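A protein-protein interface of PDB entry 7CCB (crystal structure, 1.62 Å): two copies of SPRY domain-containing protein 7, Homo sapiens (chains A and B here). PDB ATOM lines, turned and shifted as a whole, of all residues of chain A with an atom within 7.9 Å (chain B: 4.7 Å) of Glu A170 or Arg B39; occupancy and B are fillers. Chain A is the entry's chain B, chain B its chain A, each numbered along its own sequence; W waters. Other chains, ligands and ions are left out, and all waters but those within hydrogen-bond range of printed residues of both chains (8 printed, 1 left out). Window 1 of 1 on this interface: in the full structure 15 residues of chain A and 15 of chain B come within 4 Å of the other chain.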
ATOM      1  N   ARG A  39      13.310   5.290  11.932  1.00  0.00           N
ATOM      2  CA  ARG A  39      12.248   5.086  10.902  1.00  0.00           C
ATOM      3  C   ARG A  39      12.791   5.134   9.484  1.00  0.00           C
ATOM      4  O   ARG A  39      12.093   4.642   8.590  1.00  0.00           O
ATOM      5  CB  ARG A  39      11.109   6.080  11.084  1.00  0.00           C
ATOM      6  CG  ARG A  39      10.346   5.792  12.372  1.00  0.00           C
ATOM      7  CD  ARG A  39       9.012   6.478  12.458  1.00  0.00           C
ATOM      8  NE  ARG A  39       8.298   6.104  11.266  1.00  0.00           N
ATOM      9  CZ  ARG A  39       7.544   6.933  10.577  1.00  0.00           C
ATOM     10  NH1 ARG A  39       7.245   8.135  11.058  1.00  0.00           N
ATOM     11  NH2 ARG A  39       7.078   6.544   9.404  1.00  0.00           N
ATOM     12  N   TYR A  59       1.729  -7.450  10.301  1.00  0.00           N
ATOM     13  CA  TYR A  59       1.664  -6.475   9.194  1.00  0.00           C
ATOM     14  C   TYR A  59       2.654  -5.348   9.475  1.00  0.00           C
ATOM     15  O   TYR A  59       2.795  -4.934  10.629  1.00  0.00           O
ATOM     16  CB  TYR A  59       0.287  -5.850   9.097  1.00  0.00           C
ATOM     17  CG  TYR A  59       0.167  -4.768   8.058  1.00  0.00           C
ATOM     18  CD1 TYR A  59       0.244  -5.035   6.703  1.00  0.00           C
ATOM     19  CD2 TYR A  59      -0.087  -3.469   8.461  1.00  0.00           C
ATOM     20  CE1 TYR A  59       0.071  -4.045   5.752  1.00  0.00           C
ATOM     21  CE2 TYR A  59      -0.256  -2.466   7.524  1.00  0.00           C
ATOM     22  CZ  TYR A  59      -0.139  -2.740   6.180  1.00  0.00           C
ATOM     23  OH  TYR A  59      -0.327  -1.742   5.246  1.00  0.00           O
ATOM     24  N   GLU A  61       4.802  -1.845   7.191  1.00  0.00           N
ATOM     25  CA  GLU A  61       4.791  -1.059   5.944  1.00  0.00           C
ATOM     26  C   GLU A  61       6.115  -0.361   5.734  1.00  0.00           C
ATOM     27  O   GLU A  61       6.770   0.022   6.715  1.00  0.00           O
ATOM     28  CB  GLU A  61       3.777   0.080   6.031  1.00  0.00           C
ATOM     29  CG  GLU A  61       2.350  -0.289   6.001  1.00  0.00           C
ATOM     30  CD  GLU A  61       1.407   0.894   6.133  1.00  0.00           C
ATOM     31  OE1 GLU A  61       1.848   2.024   6.454  1.00  0.00           O
ATOM     32  OE2 GLU A  61       0.215   0.650   5.930  1.00  0.00           O
ATOM     33  N   LYS A  63       7.275   3.140   3.300  1.00  0.00           N
ATOM     34  CA  LYS A  63       6.985   4.153   2.279  1.00  0.00           C
ATOM     35  C   LYS A  63       8.253   4.358   1.455  1.00  0.00           C
ATOM     36  O   LYS A  63       9.359   4.490   2.005  1.00  0.00           O
ATOM     37  CB  LYS A  63       6.510   5.460   2.900  1.00  0.00           C
ATOM     38  CG  LYS A  63       6.226   6.545   1.872  1.00  0.00           C
ATOM     39  CD  LYS A  63       5.145   7.481   2.256  1.00  0.00           C
ATOM     40  CE  LYS A  63       4.955   8.531   1.179  1.00  0.00           C
ATOM     41  NZ  LYS A  63       4.517   9.794   1.800  1.00  0.00           N
ATOM     42  N   VAL A 122       3.220   3.232  -0.727  1.00  0.00           N
ATOM     43  CA  VAL A 122       3.358   2.484   0.557  1.00  0.00           C
ATOM     44  C   VAL A 122       3.249   1.008   0.239  1.00  0.00           C
ATOM     45  O   VAL A 122       2.231   0.605  -0.308  1.00  0.00           O
ATOM     46  CB  VAL A 122       2.328   2.919   1.610  1.00  0.00           C
ATOM     47  CG1 VAL A 122       2.365   2.048   2.866  1.00  0.00           C
ATOM     48  CG2 VAL A 122       2.475   4.408   1.936  1.00  0.00           C
ATOM     49  N   CYS A 166       9.894   3.344   7.510  1.00  0.00           N
ATOM     50  CA  CYS A 166       9.103   2.244   8.075  1.00  0.00           C
ATOM     51  C   CYS A 166       7.874   2.789   8.803  1.00  0.00           C
ATOM     52  O   CYS A 166       7.940   3.847   9.419  1.00  0.00           O
ATOM     53  CB  CYS A 166       9.911   1.363   9.010  1.00  0.00           C
ATOM     54  SG  CYS A 166      10.373   2.129  10.591  1.00  0.00           S
ATOM     55  N   GLN A 167       6.799   1.999   8.783  1.00  0.00           N
ATOM     56  CA  GLN A 167       5.635   2.141   9.675  1.00  0.00           C
ATOM     57  C   GLN A 167       5.440   0.774  10.337  1.00  0.00           C
ATOM     58  O   GLN A 167       5.034  -0.181   9.660  1.00  0.00           O
ATOM     59  CB  GLN A 167       4.373   2.619   8.964  1.00  0.00           C
ATOM     60  CG  GLN A 167       4.477   4.010   8.350  1.00  0.00           C
ATOM     61  CD  GLN A 167       5.229   4.078   7.040  1.00  0.00           C
ATOM     62  OE1 GLN A 167       6.187   4.867   6.847  1.00  0.00           O
ATOM     63  NE2 GLN A 167       4.739   3.325   6.066  1.00  0.00           N
ATOM     64  N   PHE A 168       5.754   0.679  11.627  1.00  0.00           N
ATOM     65  CA  PHE A 168       5.526  -0.557  12.398  1.00  0.00           C
ATOM     66  C   PHE A 168       4.285  -0.446  13.262  1.00  0.00           C
ATOM     67  O   PHE A 168       3.889  -1.470  13.810  1.00  0.00           O
ATOM     68  CB  PHE A 168       6.764  -0.935  13.211  1.00  0.00           C
ATOM     69  CG  PHE A 168       7.875  -1.465  12.348  1.00  0.00           C
ATOM     70  CD1 PHE A 168       7.723  -2.671  11.664  1.00  0.00           C
ATOM     71  CD2 PHE A 168       9.029  -0.733  12.166  1.00  0.00           C
ATOM     72  CE1 PHE A 168       8.733  -3.158  10.832  1.00  0.00           C
ATOM     73  CE2 PHE A 168      10.036  -1.211  11.339  1.00  0.00           C
ATOM     74  CZ  PHE A 168       9.868  -2.404  10.654  1.00  0.00           C
ATOM     75  N   SER A 169       3.688   0.728  13.393  1.00  0.00           N
ATOM     76  CA  SER A 169       2.493   0.847  14.260  1.00  0.00           C
ATOM     77  C   SER A 169       1.474   1.854  13.735  1.00  0.00           C
ATOM     78  O   SER A 169       0.277   1.569  13.793  1.00  0.00           O
ATOM     79  CB  SER A 169       2.921   1.166  15.648  1.00  0.00           C
ATOM     80  OG  SER A 169       3.530   2.428  15.687  1.00  0.00           O
ATOM     81  N   GLU A 170       1.904   3.001  13.232  1.00  0.00           N
ATOM     82  CA  GLU A 170       0.974   4.067  12.804  1.00  0.00           C
ATOM     83  C   GLU A 170       0.842   3.989  11.281  1.00  0.00           C
ATOM     84  O   GLU A 170       1.543   4.695  10.578  1.00  0.00           O
ATOM     85  CB  GLU A 170       1.466   5.401  13.367  1.00  0.00           C
ATOM     86  CG  GLU A 170       0.410   6.452  13.241  1.00  0.00           C
ATOM     87  CD  GLU A 170       0.750   7.823  13.809  1.00  0.00           C
ATOM     88  OE1 GLU A 170       1.931   8.046  14.159  1.00  0.00           O
ATOM     89  OE2 GLU A 170      -0.210   8.671  13.856  1.00  0.00           O
ATOM     90  N   PHE A 171       0.012   3.088  10.774  1.00  0.00           N
ATOM     91  CA  PHE A 171       0.063   2.678   9.351  1.00  0.00           C
ATOM     92  C   PHE A 171      -0.660   3.682   8.470  1.00  0.00           C
ATOM     93  O   PHE A 171      -1.661   4.330   8.912  1.00  0.00           O
ATOM     94  CB  PHE A 171      -0.588   1.305   9.180  1.00  0.00           C
ATOM     95  CG  PHE A 171       0.042   0.255  10.045  1.00  0.00           C
ATOM     96  CD1 PHE A 171       1.385  -0.009   9.916  1.00  0.00           C
ATOM     97  CD2 PHE A 171      -0.672  -0.409  11.017  1.00  0.00           C
ATOM     98  CE1 PHE A 171       2.012  -0.964  10.696  1.00  0.00           C
ATOM     99  CE2 PHE A 171      -0.052  -1.380  11.794  1.00  0.00           C
ATOM    100  CZ  PHE A 171       1.287  -1.659  11.627  1.00  0.00           C
ATOM    101  N   TYR A 172      -0.250   3.781   7.220  1.00  0.00           N
ATOM    102  CA  TYR A 172      -1.013   4.524   6.195  1.00  0.00           C
ATOM    103  C   TYR A 172      -2.248   3.768   5.738  1.00  0.00           C
ATOM    104  O   TYR A 172      -3.136   4.361   5.136  1.00  0.00           O
ATOM    105  CB  TYR A 172      -0.090   4.823   5.028  1.00  0.00           C
ATOM    106  CG  TYR A 172       0.815   6.006   5.224  1.00  0.00           C
ATOM    107  CD1 TYR A 172       0.243   7.260   5.273  1.00  0.00           C
ATOM    108  CD2 TYR A 172       2.189   5.908   5.332  1.00  0.00           C
ATOM    109  CE1 TYR A 172       1.004   8.404   5.367  1.00  0.00           C
ATOM    110  CE2 TYR A 172       2.979   7.061   5.420  1.00  0.00           C
ATOM    111  CZ  TYR A 172       2.371   8.306   5.426  1.00  0.00           C
ATOM    112  OH  TYR A 172       3.030   9.521   5.487  1.00  0.00           O
ATOM    113  N   HIS A 173      -2.249   2.454   5.957  1.00  0.00           N
ATOM    114  CA  HIS A 173      -3.343   1.549   5.536  1.00  0.00           C
ATOM    115  C   HIS A 173      -3.746   0.705   6.719  1.00  0.00           C
ATOM    116  O   HIS A 173      -2.867   0.143   7.390  1.00  0.00           O
ATOM    117  CB  HIS A 173      -2.883   0.743   4.320  1.00  0.00           C
ATOM    118  CG  HIS A 173      -2.722   1.642   3.150  1.00  0.00           C
ATOM    119  ND1 HIS A 173      -1.503   2.121   2.697  1.00  0.00           N
ATOM    120  CD2 HIS A 173      -3.676   2.271   2.417  1.00  0.00           C
ATOM    121  CE1 HIS A 173      -1.718   2.991   1.723  1.00  0.00           C
ATOM    122  NE2 HIS A 173      -3.030   3.061   1.528  1.00  0.00           N
ATOM    123  N   LYS A 181      -0.132  -5.265  14.047  1.00  0.00           N
ATOM    124  CA  LYS A 181       1.221  -4.715  14.193  1.00  0.00           C
ATOM    125  C   LYS A 181       2.053  -5.716  14.992  1.00  0.00           C
ATOM    126  O   LYS A 181       1.521  -6.526  15.789  1.00  0.00           O
ATOM    127  CB  LYS A 181       1.204  -3.348  14.878  1.00  0.00           C
ATOM    128  CG  LYS A 181       0.861  -3.378  16.349  1.00  0.00           C
ATOM    129  CD  LYS A 181       0.830  -1.997  16.940  1.00  0.00           C
ATOM    130  CE  LYS A 181       0.180  -2.052  18.304  1.00  0.00           C
ATOM    131  NZ  LYS A 181       0.545  -0.867  19.116  1.00  0.00           N
ATOM    132  N   VAL B  21      -5.082   7.931  17.816  1.00  0.00           N
ATOM    133  CA  VAL B  21      -5.388   9.359  17.579  1.00  0.00           C
ATOM    134  C   VAL B  21      -5.135   9.609  16.108  1.00  0.00           C
ATOM    135  O   VAL B  21      -4.096   9.176  15.619  1.00  0.00           O
ATOM    136  CB  VAL B  21      -4.526  10.261  18.464  1.00  0.00           C
ATOM    137  CG1 VAL B  21      -4.775  11.730  18.181  1.00  0.00           C
ATOM    138  CG2 VAL B  21      -4.778   9.894  19.942  1.00  0.00           C
ATOM    139  N   LEU B  23      -6.874  12.012  12.358  1.00  0.00           N
ATOM    140  CA  LEU B  23      -7.720  13.140  11.882  1.00  0.00           C
ATOM    141  C   LEU B  23      -9.191  12.716  11.965  1.00  0.00           C
ATOM    142  O   LEU B  23      -9.518  11.592  11.520  1.00  0.00           O
ATOM    143  CB  LEU B  23      -7.259  13.512  10.486  1.00  0.00           C
ATOM    144  CG  LEU B  23      -5.798  13.942  10.437  1.00  0.00           C
ATOM    145  CD1 LEU B  23      -5.394  14.240   9.021  1.00  0.00           C
ATOM    146  CD2 LEU B  23      -5.493  15.134  11.340  1.00  0.00           C
ATOM    147  N   VAL B  35      -7.664  10.787   4.108  1.00  0.00           N
ATOM    148  CA  VAL B  35      -7.369   9.472   3.511  1.00  0.00           C
ATOM    149  C   VAL B  35      -6.195   8.838   4.271  1.00  0.00           C
ATOM    150  O   VAL B  35      -5.682   9.427   5.271  1.00  0.00           O
ATOM    151  CB  VAL B  35      -7.059   9.655   2.028  1.00  0.00           C
ATOM    152  CG1 VAL B  35      -8.316   9.936   1.208  1.00  0.00           C
ATOM    153  CG2 VAL B  35      -5.973  10.690   1.765  1.00  0.00           C
ATOM    154  N   LYS B  36      -5.771   7.656   3.810  1.00  0.00           N
ATOM    155  CA  LYS B  36      -4.579   6.971   4.380  1.00  0.00           C
ATOM    156  C   LYS B  36      -4.809   6.727   5.884  1.00  0.00           C
ATOM    157  O   LYS B  36      -3.992   7.147   6.710  1.00  0.00           O
ATOM    158  CB  LYS B  36      -3.294   7.738   4.115  1.00  0.00           C
ATOM    159  CG  LYS B  36      -3.060   8.171   2.687  1.00  0.00           C
ATOM    160  CD  LYS B  36      -2.817   7.093   1.747  1.00  0.00           C
ATOM    161  CE  LYS B  36      -2.372   7.651   0.394  1.00  0.00           C
ATOM    162  NZ  LYS B  36      -2.575   6.637  -0.660  1.00  0.00           N
ATOM    163  N   ASN B  37      -5.880   5.994   6.248  1.00  0.00           N
ATOM    164  CA  ASN B  37      -6.042   5.462   7.619  1.00  0.00           C
ATOM    165  C   ASN B  37      -6.079   6.634   8.606  1.00  0.00           C
ATOM    166  O   ASN B  37      -5.464   6.548   9.702  1.00  0.00           O
ATOM    167  CB  ASN B  37      -4.939   4.469   7.949  1.00  0.00           C
ATOM    168  CG  ASN B  37      -5.241   3.622   9.166  1.00  0.00           C
ATOM    169  OD1 ASN B  37      -6.399   3.434   9.504  1.00  0.00           O
ATOM    170  ND2 ASN B  37      -4.210   3.282   9.904  1.00  0.00           N
ATOM    171  N   GLY B  38      -6.725   7.733   8.207  1.00  0.00           N
ATOM    172  CA  GLY B  38      -6.902   8.899   9.079  1.00  0.00           C
ATOM    173  C   GLY B  38      -5.644   9.716   9.273  1.00  0.00           C
ATOM    174  O   GLY B  38      -5.600  10.530  10.193  1.00  0.00           O
ATOM    175  N   ARG B  39      -4.660   9.578   8.398  1.00  0.00           N
ATOM    176  CA  ARG B  39      -3.358  10.255   8.610  1.00  0.00           C
ATOM    177  C   ARG B  39      -3.122  11.399   7.621  1.00  0.00           C
ATOM    178  O   ARG B  39      -2.259  12.233   7.913  1.00  0.00           O
ATOM    179  CB  ARG B  39      -2.204   9.269   8.492  1.00  0.00           C
ATOM    180  CG  ARG B  39      -2.200   8.251   9.639  1.00  0.00           C
ATOM    181  CD  ARG B  39      -0.927   7.451   9.694  1.00  0.00           C
ATOM    182  NE  ARG B  39       0.196   8.363   9.729  1.00  0.00           N
ATOM    183  CZ  ARG B  39       1.365   8.158   9.196  1.00  0.00           C
ATOM    184  NH1 ARG B  39       1.695   6.971   8.716  1.00  0.00           N
ATOM    185  NH2 ARG B  39       2.241   9.153   9.167  1.00  0.00           N
ATOM    186  N   ARG B  40      -3.801  11.432   6.488  1.00  0.00           N
ATOM    187  CA  ARG B  40      -3.501  12.427   5.428  1.00  0.00           C
ATOM    188  C   ARG B  40      -4.685  13.359   5.251  1.00  0.00           C
ATOM    189  O   ARG B  40      -5.830  12.882   5.082  1.00  0.00           O
ATOM    190  CB  ARG B  40      -3.199  11.734   4.087  1.00  0.00           C
ATOM    191  CG  ARG B  40      -3.015  12.719   2.941  1.00  0.00           C
ATOM    192  CD  ARG B  40      -2.367  12.065   1.738  1.00  0.00           C
ATOM    193  NE  ARG B  40      -0.987  11.803   2.029  1.00  0.00           N
ATOM    194  CZ  ARG B  40      -0.132  11.273   1.174  1.00  0.00           C
ATOM    195  NH1 ARG B  40      -0.568  10.870  -0.009  1.00  0.00           N
ATOM    196  NH2 ARG B  40       1.113  11.066   1.546  1.00  0.00           N
ATOM    197  N   ILE B  41      -4.399  14.658   5.254  1.00  0.00           N
ATOM    198  CA  ILE B  41      -5.378  15.689   4.915  1.00  0.00           C
ATOM    199  C   ILE B  41      -5.000  16.326   3.588  1.00  0.00           C
ATOM    200  O   ILE B  41      -3.865  16.751   3.388  1.00  0.00           O
ATOM    201  CB  ILE B  41      -5.555  16.718   6.050  1.00  0.00           C
ATOM    202  CG1 ILE B  41      -6.588  17.760   5.626  1.00  0.00           C
ATOM    203  CG2 ILE B  41      -4.255  17.314   6.532  1.00  0.00           C
ATOM    204  CD1 ILE B  41      -6.958  18.773   6.704  1.00  0.00           C
ATOM    205  N   LEU B 164      -0.830  17.252   4.001  1.00  0.00           N
ATOM    206  CA  LEU B 164      -0.080  17.057   5.266  1.00  0.00           C
ATOM    207  C   LEU B 164      -0.421  15.676   5.812  1.00  0.00           C
ATOM    208  O   LEU B 164      -1.598  15.276   5.770  1.00  0.00           O
ATOM    209  CB  LEU B 164      -0.450  18.151   6.269  1.00  0.00           C
ATOM    210  CG  LEU B 164       0.420  19.408   6.250  1.00  0.00           C
ATOM    211  CD1 LEU B 164       0.401  20.140   4.920  1.00  0.00           C
ATOM    212  CD2 LEU B 164       0.047  20.351   7.388  1.00  0.00           C
ATOM    213  N   ASP B 165       0.589  14.990   6.362  1.00  0.00           N
ATOM    214  CA  ASP B 165       0.413  13.662   6.987  1.00  0.00           C
ATOM    215  C   ASP B 165       0.726  13.807   8.459  1.00  0.00           C
ATOM    216  O   ASP B 165       1.767  14.401   8.819  1.00  0.00           O
ATOM    217  CB  ASP B 165       1.322  12.595   6.392  1.00  0.00           C
ATOM    218  CG  ASP B 165       0.996  12.303   4.945  1.00  0.00           C
ATOM    219  OD1 ASP B 165      -0.080  12.720   4.510  1.00  0.00           O
ATOM    220  OD2 ASP B 165       1.857  11.671   4.286  1.00  0.00           O
ATOM    221  N   CYS B 166      -0.150  13.310   9.293  1.00  0.00           N
ATOM    222  CA  CYS B 166       0.062  13.376  10.757  1.00  0.00           C
ATOM    223  C   CYS B 166       0.890  12.203  11.265  1.00  0.00           C
ATOM    224  O   CYS B 166       0.777  11.110  10.753  1.00  0.00           O
ATOM    225  CB  CYS B 166      -1.257  13.433  11.510  1.00  0.00           C
ATOM    226  SG  CYS B 166      -2.264  11.917  11.488  1.00  0.00           S
ATOM    227  N   GLN B 167       1.625  12.454  12.355  1.00  0.00           N
ATOM    228  CA  GLN B 167       2.213  11.383  13.210  1.00  0.00           C
ATOM    229  C   GLN B 167       1.761  11.703  14.626  1.00  0.00           C
ATOM    230  O   GLN B 167       2.198  12.733  15.213  1.00  0.00           O
ATOM    231  CB  GLN B 167       3.742  11.279  13.065  1.00  0.00           C
ATOM    232  CG  GLN B 167       4.269  10.872  11.694  1.00  0.00           C
ATOM    233  CD  GLN B 167       4.291  11.974  10.645  1.00  0.00           C
ATOM    234  OE1 GLN B 167       3.706  11.884   9.539  1.00  0.00           O
ATOM    235  NE2 GLN B 167       5.028  13.031  10.968  1.00  0.00           N
ATOM    236  N   PHE B 168       0.865  10.904  15.180  1.00  0.00           N
ATOM    237  CA  PHE B 168       0.412  11.065  16.571  1.00  0.00           C
ATOM    238  C   PHE B 168       1.098  10.068  17.496  1.00  0.00           C
ATOM    239  O   PHE B 168       0.905  10.190  18.689  1.00  0.00           O
ATOM    240  CB  PHE B 168      -1.110  11.035  16.681  1.00  0.00           C
ATOM    241  CG  PHE B 168      -1.743  12.267  16.118  1.00  0.00           C
ATOM    242  CD1 PHE B 168      -1.640  13.463  16.812  1.00  0.00           C
ATOM    243  CD2 PHE B 168      -2.517  12.201  14.978  1.00  0.00           C
ATOM    244  CE1 PHE B 168      -2.214  14.610  16.287  1.00  0.00           C
ATOM    245  CE2 PHE B 168      -3.137  13.352  14.483  1.00  0.00           C
ATOM    246  CZ  PHE B 168      -2.954  14.547  15.142  1.00  0.00           C
ATOM    247  N   SER B 169       1.815   9.068  16.981  1.00  0.00           N
ATOM    248  CA  SER B 169       2.445   8.069  17.884  1.00  0.00           C
ATOM    249  C   SER B 169       3.812   7.628  17.364  1.00  0.00           C
ATOM    250  O   SER B 169       4.743   7.545  18.185  1.00  0.00           O
ATOM    251  CB  SER B 169       1.537   6.895  18.147  1.00  0.00           C
ATOM    252  OG  SER B 169       1.231   6.241  16.931  1.00  0.00           O
ATOM    253  N   GLU B 170       3.951   7.330  16.075  1.00  0.00           N
ATOM    254  CA  GLU B 170       5.205   6.781  15.511  1.00  0.00           C
ATOM    255  C   GLU B 170       6.019   7.913  14.877  1.00  0.00           C
ATOM    256  O   GLU B 170       5.945   8.165  13.666  1.00  0.00           O
ATOM    257  CB  GLU B 170       4.888   5.645  14.548  1.00  0.00           C
ATOM    258  CG  GLU B 170       6.099   4.831  14.170  1.00  0.00           C
ATOM    259  CD  GLU B 170       5.813   3.624  13.310  1.00  0.00           C
ATOM    260  OE1 GLU B 170       4.674   3.539  12.773  1.00  0.00           O
ATOM    261  OE2 GLU B 170       6.788   2.812  13.105  1.00  0.00           O
HETATM  262  O   HOH W   1       9.233   2.855  14.139  1.00  0.00           O
HETATM  263  O   HOH W   2      -1.487   7.306  16.346  1.00  0.00           O
HETATM  264  O   HOH W   3       4.058   5.840  10.921  1.00  0.00           O
HETATM  265  O   HOH W   4      -2.813   8.457  13.305  1.00  0.00           O
HETATM  266  O   HOH W   5      -2.301   4.566  11.993  1.00  0.00           O
HETATM  267  O   HOH W   6       3.827   8.106  11.814  1.00  0.00           O
HETATM  268  O   HOH W   7       6.340   1.484  16.033  1.00  0.00           O
HETATM  269  O   HOH W   8       4.628  10.799   7.083  1.00  0.00           O
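ND2 of Asn B37 is in hydrogen-bond range of O of Phe A171, 2.9 Å away.
The backbone carbonyl oxygen (O) of Tyr A172 lies close to the backbone NH (N) of Asn B37 (3.4 Å).
The guanidinium group (NH1) of Arg B39 sits at hydrogen-bond distance from the backbone carbonyl oxygen (O) of Glu A170, at 2.9 Å.
OH of Tyr A172 lies within hydrogen-bond range of OD2 of Asp B165 (2.7 Å).
N of Phe B168 lies within hydrogen-bond range of OE2 of Glu A170.
The side-chain carboxylate (OE1) of Glu A170 lies within hydrogen-bond range of the backbone NH (N) of Ser B169 (3.0 Å).
The backbone carbonyl oxygen (O) of Glu B170 sits at hydrogen-bond distance from the guanidinium group (NH1) of Arg A39 (2.9 Å).
The side-chain carboxylate (OE2) of Glu B170 sits at hydrogen-bond distance from the backbone NH (N) of Phe A168 (2.8 Å).
The backbone NH (N) of Ser A169 lies within hydrogen-bond range of the side-chain carboxylate (OE1) of Glu B170.
The side-chain carboxylate (OE1) of Glu B170 is in hydrogen-bond range of the backbone NH (N) of Glu A170 (2.9 Å).
The backbone carbonyl oxygen (O) of Tyr A172 sits close to the backbone carbonyl oxygen (O) of Lys B36 (3.3 Å).
N of Cys B166 sits at hydrogen-bond distance from O of Arg B39, 2.7 Å away.
OD1 of Asp B165 lies within salt-bridge range of NE of Arg B40 (2.8 Å).
The backbone carbonyl oxygen (O) of Asp B165 lies close to the side-chain amide oxygen (OE1) of Gln B167, at 3.3 Å.
N of Cys A166 sits at hydrogen-bond distance from O of Arg A39, 2.8 Å away.
The side-chain amide oxygen (OE1) of Gln A167 lies within hydrogen-bond range of the guanidinium group (NH2) of Arg A39.
OE1 of Glu A61 lies within hydrogen-bond range of N of Tyr A172 (2.8 Å).
Among the printed residues, merely in contact across the chains: Lys A63 with Arg B40, Cys A166 with Glu B170, Gln A167 with Glu B170, Glu A170 with Gln B167, Phe A171 with Arg B39, Tyr A172 with Arg B39 and His A173 with Asn B37.
Of chain B, only Arg B39 (2.9 Å), Gln B167 (3.5 Å), Phe B168 (2.8 Å), Ser B169 (3.0 Å) and Glu B170 (2.9 Å) come within 4 Å of Glu A170.
Arg B39 touches three residues of chain A.
Printed residues of chain B within 4 Å of Phe A171: Asn B37 (2.9 Å) and Arg B39 (3.3 Å).
Printed residues of chain B within 4 Å of Arg A39: Glu B170.
Printed residues of chain B within 4 Å of Phe A168: Glu B170 (2.8 Å).
The nearest residue of chain A that does not touch Arg B39 is Gln A167 (4.1 Å).
The nearest printed residue of chain B that does not touch Tyr A172 is Arg B40 (4.6 Å).
Of the 16 printed residues of chain B, 9 touch a printed residue of chain A.
Hydrophobic or aromatic side chains of chain B that line the printed part of chain A: Phe B168.
Printed residues of chain A that touch a printed residue of chain B: Arg A39, Lys A63, Cys A166, Gln A167, Phe A168, Ser A169, Glu A170, Phe A171, Tyr A172 and His A173.
Hydrophobic or aromatic side chains of chain A within 4 Å of the printed part of chain B: Phe A168 and Tyr A172.
Among the printed residues, no Asp or Glu carboxylate lies within 4 Å of a Lys or Arg side-chain nitrogen of the other chain.
Arg A39 touches Glu B170, and with the chains exchanged Glu A170 touches Arg B39.
Cys A166 touches Glu B170, but with the chains exchanged Glu A170 does not touch Cys B166 (4.1 Å).
Phe A168 touches Glu B170, and with the chains exchanged Glu A170 touches Phe B168.
Glu B170 touches its own counterpart, Glu A170.
Of the 18 pairs that touch across the chains among the printed residues, 9 have their exchanged pair printed and touching as well.
Water W8 lies within hydrogen-bond range of the side-chain hydroxyl of Tyr A172 (2.6 Å) and the side-chain amide oxygen of Gln B167 (2.8 Å).
Water W1 bridges the side-chain carboxylate (OE2) of Glu B170 (2.7 Å) and the side-chain sulfur (SG) of Cys A166 (3.8 Å).
Water W4 bridges OE2 of Glu A170 (2.7 Å) and O of Val B21 (2.7 Å).
Water W3 lies within hydrogen-bond range of the backbone carbonyl oxygen of Glu A170, the side-chain carboxylate of Glu B170, the guanidinium group of Arg B39 and the guanidinium group of Arg A39.
Water W2 lies within hydrogen-bond range of the side-chain hydroxyl (OG) of Ser B169 (3.0 Å), the side-chain carboxylate (OE2) of Glu A170 (3.1 Å) and the backbone carbonyl oxygen (O) of Val B21 (3.3 Å).
Water W7 lies within hydrogen-bond range of the side-chain hydroxyl (OG) of Ser A169 (3.0 Å) and the side-chain carboxylate (OE2) of Glu B170 (3.2 Å).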
